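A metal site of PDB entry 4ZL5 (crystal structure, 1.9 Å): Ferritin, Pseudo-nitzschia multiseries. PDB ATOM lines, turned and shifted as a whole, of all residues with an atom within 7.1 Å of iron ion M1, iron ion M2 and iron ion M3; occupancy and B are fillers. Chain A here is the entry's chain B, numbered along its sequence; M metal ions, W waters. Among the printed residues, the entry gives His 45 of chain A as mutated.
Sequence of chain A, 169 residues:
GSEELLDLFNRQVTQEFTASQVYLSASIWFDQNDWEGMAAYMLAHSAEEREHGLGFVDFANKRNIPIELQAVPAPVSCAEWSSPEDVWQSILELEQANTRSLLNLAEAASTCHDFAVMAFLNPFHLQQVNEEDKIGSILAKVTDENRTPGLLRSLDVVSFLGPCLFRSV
A ring nitrogen (ND1) of His 52 sits close to the backbone carbonyl oxygen of Glu 48.
OE1 of Glu 95 is in hydrogen-bond range of ND2 of Asn 98.
OH of Tyr 23 lies close to OE2 of Glu 95 (2.7 Å).
The side-chain carboxylate (OE1) of Glu 95 is in hydrogen-bond range of the side-chain amide nitrogen (NE2) of Gln 128, at 2.9 Å.
OE2 of Glu 16 sits at hydrogen-bond distance from NE2 of Gln 12, 2.9 Å away.
OE1 of Gln 127 sits close to OE2 of Glu 48 (2.7 Å).
ND1 of His 45 sits close to OH of Tyr 23 (3.5 Å).
The side-chain amide oxygen of Asn 98 sits at hydrogen-bond distance from the side-chain amide nitrogen of Gln 15 (2.9 Å).
Of the 21 residues printed, 4 come within 4 Å of iron ion M1.
Four residues have an atom within 4 Å of iron ion M2: Glu 48, His 52, Gln 127 and Glu 131.
Residues that only touch iron ion M3: Asn 98 (3.5 Å).
Within 4 Å of iron ion M3: Glu 16, Glu 49, His 52 and Asn 98.
The nearest printed residue that does not touch iron ion M3 is Gln 128 (4.1 Å).
Iron ion M1 is bound by water W3 (2.0 Å), the side-chain carboxylate of Glu 131 (2.0 Å), the side-chain carboxylate of Glu 49 (2.1 Å), the side-chain carboxylate of Glu 95 (2.2 Å), water W1 (2.2 Å) and a ring nitrogen (NE2) of His 45 (2.4 Å).
Iron ion M2 is bound by OE2 of Glu 131 (1.8 Å).
A ring nitrogen (NE2) of His 52 is bound to iron ion M2 (2.0 Å).
Water W3 binds iron ion M2 (2.2 Å).
OE1 of Gln 127 binds iron ion M2, at 2.3 Å.
Slightly farther from iron ion M2 lies the side-chain carboxylate (OE2) of Glu 48 (2.7 Å).
Iron ion M3 is bound by the side-chain carboxylate (OE1) of Glu 49 (2.0 Å), the side-chain carboxylate (OE1) of Glu 16 (2.2 Å), water W1 (2.3 Å) and water W2 (2.3 Å).
Iron ion M3 has four donor atoms within binding distance.
Water W1 lies within hydrogen-bond range of OE1 of Gln 128 (2.6 Å), OE1 of Glu 95 (2.6 Å) and ND2 of Asn 98 (3.3 Å).
Water W2 bridges OE2 of Glu 16 (2.7 Å) and OE1 of Gln 128 (3.5 Å).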
ATOM      1  N   GLN A  12     -22.533 -37.757 -20.075  1.00  0.00           N
ATOM      2  CA  GLN A  12     -22.174 -36.350 -19.933  1.00  0.00           C
ATOM      3  C   GLN A  12     -23.053 -35.686 -18.910  1.00  0.00           C
ATOM      4  O   GLN A  12     -22.607 -34.838 -18.177  1.00  0.00           O
ATOM      5  CB  GLN A  12     -22.318 -35.623 -21.254  1.00  0.00           C
ATOM      6  CG  GLN A  12     -21.788 -34.217 -21.228  1.00  0.00           C
ATOM      7  CD  GLN A  12     -20.289 -34.169 -20.936  1.00  0.00           C
ATOM      8  OE1 GLN A  12     -19.546 -35.094 -21.308  1.00  0.00           O
ATOM      9  NE2 GLN A  12     -19.863 -33.136 -20.273  1.00  0.00           N
ATOM     10  N   GLN A  15     -21.713 -36.566 -15.623  1.00  0.00           N
ATOM     11  CA  GLN A  15     -20.515 -35.813 -15.384  1.00  0.00           C
ATOM     12  C   GLN A  15     -20.858 -34.393 -14.905  1.00  0.00           C
ATOM     13  O   GLN A  15     -20.184 -33.917 -14.029  1.00  0.00           O
ATOM     14  CB  GLN A  15     -19.632 -35.781 -16.651  1.00  0.00           C
ATOM     15  CG  GLN A  15     -18.321 -35.048 -16.560  1.00  0.00           C
ATOM     16  CD  GLN A  15     -17.391 -35.641 -15.482  1.00  0.00           C
ATOM     17  OE1 GLN A  15     -17.393 -36.887 -15.283  1.00  0.00           O
ATOM     18  NE2 GLN A  15     -16.613 -34.757 -14.750  1.00  0.00           N
ATOM     19  N   GLU A  16     -21.841 -33.755 -15.524  1.00  0.00           N
ATOM     20  CA  GLU A  16     -22.196 -32.393 -15.115  1.00  0.00           C
ATOM     21  C   GLU A  16     -22.763 -32.380 -13.719  1.00  0.00           C
ATOM     22  O   GLU A  16     -22.388 -31.512 -12.938  1.00  0.00           O
ATOM     23  CB  GLU A  16     -23.236 -31.791 -16.065  1.00  0.00           C
ATOM     24  CG  GLU A  16     -22.810 -31.668 -17.502  1.00  0.00           C
ATOM     25  CD  GLU A  16     -21.596 -30.750 -17.666  1.00  0.00           C
ATOM     26  OE1 GLU A  16     -21.378 -29.888 -16.808  1.00  0.00           O
ATOM     27  OE2 GLU A  16     -20.851 -30.956 -18.642  1.00  0.00           O
ATOM     28  N   ALA A  19     -19.901 -33.023 -11.316  1.00  0.00           N
ATOM     29  CA  ALA A  19     -19.168 -31.768 -11.104  1.00  0.00           C
ATOM     30  C   ALA A  19     -19.936 -30.812 -10.217  1.00  0.00           C
ATOM     31  O   ALA A  19     -19.314 -30.181  -9.341  1.00  0.00           O
ATOM     32  CB  ALA A  19     -18.809 -31.101 -12.435  1.00  0.00           C
ATOM     33  N   TYR A  23     -18.227 -29.217  -6.877  1.00  0.00           N
ATOM     34  CA  TYR A  23     -18.182 -27.799  -6.577  1.00  0.00           C
ATOM     35  C   TYR A  23     -18.883 -27.495  -5.279  1.00  0.00           C
ATOM     36  O   TYR A  23     -18.419 -26.640  -4.496  1.00  0.00           O
ATOM     37  CB  TYR A  23     -18.819 -26.991  -7.716  1.00  0.00           C
ATOM     38  CG  TYR A  23     -17.919 -26.658  -8.857  1.00  0.00           C
ATOM     39  CD1 TYR A  23     -17.023 -25.623  -8.785  1.00  0.00           C
ATOM     40  CD2 TYR A  23     -17.987 -27.328 -10.062  1.00  0.00           C
ATOM     41  CE1 TYR A  23     -16.216 -25.273  -9.855  1.00  0.00           C
ATOM     42  CE2 TYR A  23     -17.116 -27.027 -11.116  1.00  0.00           C
ATOM     43  CZ  TYR A  23     -16.259 -25.972 -10.986  1.00  0.00           C
ATOM     44  OH  TYR A  23     -15.453 -25.525 -11.967  1.00  0.00           O
ATOM     45  N   HIS A  45     -20.801 -21.867  -9.169  1.00  0.00           N
ATOM     46  CA  HIS A  45     -20.359 -22.672 -10.209  1.00  0.00           C
ATOM     47  C   HIS A  45     -21.071 -24.062 -10.072  1.00  0.00           C
ATOM     48  O   HIS A  45     -21.373 -24.660 -11.065  1.00  0.00           O
ATOM     49  CB  HIS A  45     -18.855 -22.779 -10.228  1.00  0.00           C
ATOM     50  CG  HIS A  45     -18.311 -23.137 -11.562  1.00  0.00           C
ATOM     51  ND1 HIS A  45     -17.220 -22.517 -12.130  1.00  0.00           N
ATOM     52  CD2 HIS A  45     -18.712 -24.073 -12.476  1.00  0.00           C
ATOM     53  CE1 HIS A  45     -16.938 -23.082 -13.297  1.00  0.00           C
ATOM     54  NE2 HIS A  45     -17.861 -23.992 -13.551  1.00  0.00           N
ATOM     55  N   GLU A  48     -24.244 -23.694 -11.826  1.00  0.00           N
ATOM     56  CA  GLU A  48     -24.036 -23.602 -13.241  1.00  0.00           C
ATOM     57  C   GLU A  48     -23.732 -24.978 -13.884  1.00  0.00           C
ATOM     58  O   GLU A  48     -24.215 -25.276 -15.023  1.00  0.00           O
ATOM     59  CB  GLU A  48     -22.852 -22.662 -13.502  1.00  0.00           C
ATOM     60  CG  GLU A  48     -22.313 -22.772 -14.920  1.00  0.00           C
ATOM     61  CD  GLU A  48     -21.188 -21.769 -15.167  1.00  0.00           C
ATOM     62  OE1 GLU A  48     -21.071 -20.808 -14.376  1.00  0.00           O
ATOM     63  OE2 GLU A  48     -20.412 -21.975 -16.132  1.00  0.00           O
ATOM     64  N   GLU A  49     -22.995 -25.816 -13.183  1.00  0.00           N
ATOM     65  CA  GLU A  49     -22.841 -27.210 -13.723  1.00  0.00           C
ATOM     66  C   GLU A  49     -24.167 -27.952 -13.817  1.00  0.00           C
ATOM     67  O   GLU A  49     -24.421 -28.732 -14.747  1.00  0.00           O
ATOM     68  CB  GLU A  49     -21.955 -28.036 -12.876  1.00  0.00           C
ATOM     69  CG  GLU A  49     -20.569 -27.572 -12.749  1.00  0.00           C
ATOM     70  CD  GLU A  49     -19.795 -27.548 -14.052  1.00  0.00           C
ATOM     71  OE1 GLU A  49     -20.078 -28.202 -15.044  1.00  0.00           O
ATOM     72  OE2 GLU A  49     -18.810 -26.909 -13.955  1.00  0.00           O
ATOM     73  N   ARG A  50     -24.992 -27.784 -12.786  1.00  0.00           N
ATOM     74  CA  ARG A  50     -26.309 -28.370 -12.799  1.00  0.00           C
ATOM     75  C   ARG A  50     -27.064 -27.837 -14.019  1.00  0.00           C
ATOM     76  O   ARG A  50     -27.758 -28.588 -14.731  1.00  0.00           O
ATOM     77  CB  ARG A  50     -27.107 -28.056 -11.543  1.00  0.00           C
ATOM     78  CG  ARG A  50     -28.449 -28.773 -11.541  1.00  0.00           C
ATOM     79  CD  ARG A  50     -29.052 -28.988 -10.139  1.00  0.00           C
ATOM     80  NE  ARG A  50     -30.398 -29.568 -10.217  1.00  0.00           N
ATOM     81  CZ  ARG A  50     -31.463 -28.830 -10.526  1.00  0.00           C
ATOM     82  NH1 ARG A  50     -31.346 -27.556 -10.789  1.00  0.00           N
ATOM     83  NH2 ARG A  50     -32.632 -29.390 -10.713  1.00  0.00           N
ATOM     84  N   HIS A  52     -25.830 -26.880 -16.907  1.00  0.00           N
ATOM     85  CA  HIS A  52     -25.312 -27.590 -18.067  1.00  0.00           C
ATOM     86  C   HIS A  52     -25.946 -28.983 -18.198  1.00  0.00           C
ATOM     87  O   HIS A  52     -26.354 -29.406 -19.296  1.00  0.00           O
ATOM     88  CB  HIS A  52     -23.813 -27.782 -18.034  1.00  0.00           C
ATOM     89  CG  HIS A  52     -23.033 -26.529 -17.935  1.00  0.00           C
ATOM     90  ND1 HIS A  52     -23.514 -25.320 -18.396  1.00  0.00           N
ATOM     91  CD2 HIS A  52     -21.781 -26.304 -17.470  1.00  0.00           C
ATOM     92  CE1 HIS A  52     -22.607 -24.395 -18.172  1.00  0.00           C
ATOM     93  NE2 HIS A  52     -21.548 -24.961 -17.616  1.00  0.00           N
ATOM     94  N   GLY A  53     -25.984 -29.713 -17.104  1.00  0.00           N
ATOM     95  CA  GLY A  53     -26.644 -31.004 -17.164  1.00  0.00           C
ATOM     96  C   GLY A  53     -28.078 -30.920 -17.647  1.00  0.00           C
ATOM     97  O   GLY A  53     -28.510 -31.751 -18.446  1.00  0.00           O
ATOM     98  N   PHE A  56     -28.282 -30.516 -21.374  1.00  0.00           N
ATOM     99  CA  PHE A  56     -28.141 -31.801 -22.006  1.00  0.00           C
ATOM    100  C   PHE A  56     -29.365 -32.650 -21.963  1.00  0.00           C
ATOM    101  O   PHE A  56     -29.733 -33.213 -22.986  1.00  0.00           O
ATOM    102  CB  PHE A  56     -26.946 -32.573 -21.481  1.00  0.00           C
ATOM    103  CG  PHE A  56     -25.608 -32.112 -22.088  1.00  0.00           C
ATOM    104  CD1 PHE A  56     -25.013 -30.929 -21.668  1.00  0.00           C
ATOM    105  CD2 PHE A  56     -24.984 -32.843 -23.072  1.00  0.00           C
ATOM    106  CE1 PHE A  56     -23.844 -30.452 -22.252  1.00  0.00           C
ATOM    107  CE2 PHE A  56     -23.803 -32.373 -23.666  1.00  0.00           C
ATOM    108  CZ  PHE A  56     -23.238 -31.182 -23.250  1.00  0.00           C
ATOM    109  N   LEU A  94     -11.128 -31.358 -12.367  1.00  0.00           N
ATOM    110  CA  LEU A  94     -12.506 -31.644 -12.667  1.00  0.00           C
ATOM    111  C   LEU A  94     -12.934 -31.065 -14.034  1.00  0.00           C
ATOM    112  O   LEU A  94     -13.540 -31.735 -14.883  1.00  0.00           O
ATOM    113  CB  LEU A  94     -13.313 -31.024 -11.528  1.00  0.00           C
ATOM    114  CG  LEU A  94     -14.842 -31.120 -11.640  1.00  0.00           C
ATOM    115  CD1 LEU A  94     -15.237 -32.538 -11.489  1.00  0.00           C
ATOM    116  CD2 LEU A  94     -15.556 -30.293 -10.583  1.00  0.00           C
ATOM    117  N   GLU A  95     -12.606 -29.795 -14.234  1.00  0.00           N
ATOM    118  CA  GLU A  95     -12.892 -29.161 -15.503  1.00  0.00           C
ATOM    119  C   GLU A  95     -12.124 -29.737 -16.639  1.00  0.00           C
ATOM    120  O   GLU A  95     -12.674 -29.881 -17.745  1.00  0.00           O
ATOM    121  CB  GLU A  95     -12.693 -27.657 -15.432  1.00  0.00           C
ATOM    122  CG  GLU A  95     -13.752 -26.900 -14.607  1.00  0.00           C
ATOM    123  CD  GLU A  95     -15.157 -26.927 -15.151  1.00  0.00           C
ATOM    124  OE1 GLU A  95     -15.460 -27.429 -16.253  1.00  0.00           O
ATOM    125  OE2 GLU A  95     -16.006 -26.343 -14.436  1.00  0.00           O
ATOM    126  N   ASN A  98     -14.132 -32.644 -17.425  1.00  0.00           N
ATOM    127  CA  ASN A  98     -15.386 -32.209 -18.076  1.00  0.00           C
ATOM    128  C   ASN A  98     -15.011 -32.020 -19.595  1.00  0.00           C
ATOM    129  O   ASN A  98     -15.692 -32.541 -20.511  1.00  0.00           O
ATOM    130  CB  ASN A  98     -16.015 -30.880 -17.542  1.00  0.00           C
ATOM    131  CG  ASN A  98     -16.709 -30.952 -16.120  1.00  0.00           C
ATOM    132  OD1 ASN A  98     -17.006 -32.030 -15.566  1.00  0.00           O
ATOM    133  ND2 ASN A  98     -16.964 -29.737 -15.530  1.00  0.00           N
ATOM    134  N   LEU A 102     -16.450 -33.961 -22.995  1.00  0.00           N
ATOM    135  CA  LEU A 102     -17.152 -33.303 -24.136  1.00  0.00           C
ATOM    136  C   LEU A 102     -16.536 -33.603 -25.426  1.00  0.00           C
ATOM    137  O   LEU A 102     -17.216 -33.695 -26.448  1.00  0.00           O
ATOM    138  CB  LEU A 102     -17.136 -31.784 -24.038  1.00  0.00           C
ATOM    139  CG  LEU A 102     -18.121 -31.200 -23.060  1.00  0.00           C
ATOM    140  CD1 LEU A 102     -17.810 -29.705 -22.980  1.00  0.00           C
ATOM    141  CD2 LEU A 102     -19.564 -31.398 -23.495  1.00  0.00           C
ATOM    142  N   PHE A 124     -20.576 -25.241 -25.722  1.00  0.00           N
ATOM    143  CA  PHE A 124     -19.935 -25.883 -24.590  1.00  0.00           C
ATOM    144  C   PHE A 124     -18.419 -26.060 -24.804  1.00  0.00           C
ATOM    145  O   PHE A 124     -17.638 -25.877 -23.855  1.00  0.00           O
ATOM    146  CB  PHE A 124     -20.585 -27.233 -24.295  1.00  0.00           C
ATOM    147  CG  PHE A 124     -22.037 -27.143 -23.915  1.00  0.00           C
ATOM    148  CD1 PHE A 124     -22.395 -26.865 -22.579  1.00  0.00           C
ATOM    149  CD2 PHE A 124     -23.049 -27.319 -24.852  1.00  0.00           C
ATOM    150  CE1 PHE A 124     -23.717 -26.787 -22.206  1.00  0.00           C
ATOM    151  CE2 PHE A 124     -24.391 -27.279 -24.479  1.00  0.00           C
ATOM    152  CZ  PHE A 124     -24.728 -26.963 -23.173  1.00  0.00           C
ATOM    153  N   GLN A 127     -17.145 -22.688 -23.993  1.00  0.00           N
ATOM    154  CA  GLN A 127     -17.269 -22.354 -22.574  1.00  0.00           C
ATOM    155  C   GLN A 127     -16.156 -23.059 -21.778  1.00  0.00           C
ATOM    156  O   GLN A 127     -15.576 -22.430 -20.862  1.00  0.00           O
ATOM    157  CB  GLN A 127     -18.614 -22.804 -22.023  1.00  0.00           C
ATOM    158  CG  GLN A 127     -18.709 -22.644 -20.487  1.00  0.00           C
ATOM    159  CD  GLN A 127     -20.135 -22.487 -19.974  1.00  0.00           C
ATOM    160  OE1 GLN A 127     -20.350 -22.045 -18.831  1.00  0.00           O
ATOM    161  NE2 GLN A 127     -21.127 -22.840 -20.804  1.00  0.00           N
ATOM    162  N   GLN A 128     -15.844 -24.287 -22.150  1.00  0.00           N
ATOM    163  CA  GLN A 128     -14.826 -25.094 -21.451  1.00  0.00           C
ATOM    164  C   GLN A 128     -13.460 -24.390 -21.608  1.00  0.00           C
ATOM    165  O   GLN A 128     -12.699 -24.308 -20.618  1.00  0.00           O
ATOM    166  CB  GLN A 128     -14.734 -26.551 -21.894  1.00  0.00           C
ATOM    167  CG  GLN A 128     -15.837 -27.428 -21.322  1.00  0.00           C
ATOM    168  CD  GLN A 128     -15.937 -27.273 -19.809  1.00  0.00           C
ATOM    169  OE1 GLN A 128     -16.836 -26.577 -19.290  1.00  0.00           O
ATOM    170  NE2 GLN A 128     -14.903 -27.746 -19.111  1.00  0.00           N
ATOM    171  N   GLU A 131     -13.563 -21.548 -19.116  1.00  0.00           N
ATOM    172  CA  GLU A 131     -13.493 -22.039 -17.733  1.00  0.00           C
ATOM    173  C   GLU A 131     -12.152 -22.529 -17.323  1.00  0.00           C
ATOM    174  O   GLU A 131     -11.696 -22.153 -16.253  1.00  0.00           O
ATOM    175  CB  GLU A 131     -14.544 -23.151 -17.480  1.00  0.00           C
ATOM    176  CG  GLU A 131     -15.895 -22.487 -17.463  1.00  0.00           C
ATOM    177  CD  GLU A 131     -17.044 -23.420 -17.048  1.00  0.00           C
ATOM    178  OE1 GLU A 131     -16.720 -24.467 -16.502  1.00  0.00           O
ATOM    179  OE2 GLU A 131     -18.214 -23.097 -17.356  1.00  0.00           O
ATOM    180  N   ILE A 135     -10.072 -20.824 -14.241  1.00  0.00           N
ATOM    181  CA  ILE A 135      -9.719 -21.588 -13.032  1.00  0.00           C
ATOM    182  C   ILE A 135      -8.182 -21.767 -12.959  1.00  0.00           C
ATOM    183  O   ILE A 135      -7.577 -21.715 -11.894  1.00  0.00           O
ATOM    184  CB  ILE A 135     -10.446 -22.947 -13.019  1.00  0.00           C
ATOM    185  CG1 ILE A 135     -11.951 -22.729 -13.005  1.00  0.00           C
ATOM    186  CG2 ILE A 135      -9.984 -23.808 -11.870  1.00  0.00           C
ATOM    187  CD1 ILE A 135     -12.715 -23.952 -13.444  1.00  0.00           C
HETATM  188 FE    FE M   1     -17.878 -25.606 -15.274  1.00  0.00          FE
HETATM  189 FE    FE M   2     -19.774 -23.990 -17.760  1.00  0.00          FE
HETATM  190 FE    FE M   3     -19.824 -28.303 -16.992  1.00  0.00          FE
HETATM  191  O   HOH W   1     -17.942 -26.990 -16.978  1.00  0.00           O
HETATM  192  O   HOH W   2     -19.683 -28.563 -19.289  1.00  0.00           O
HETATM  193  O   HOH W   3     -19.535 -24.580 -15.652  1.00  0.00           O
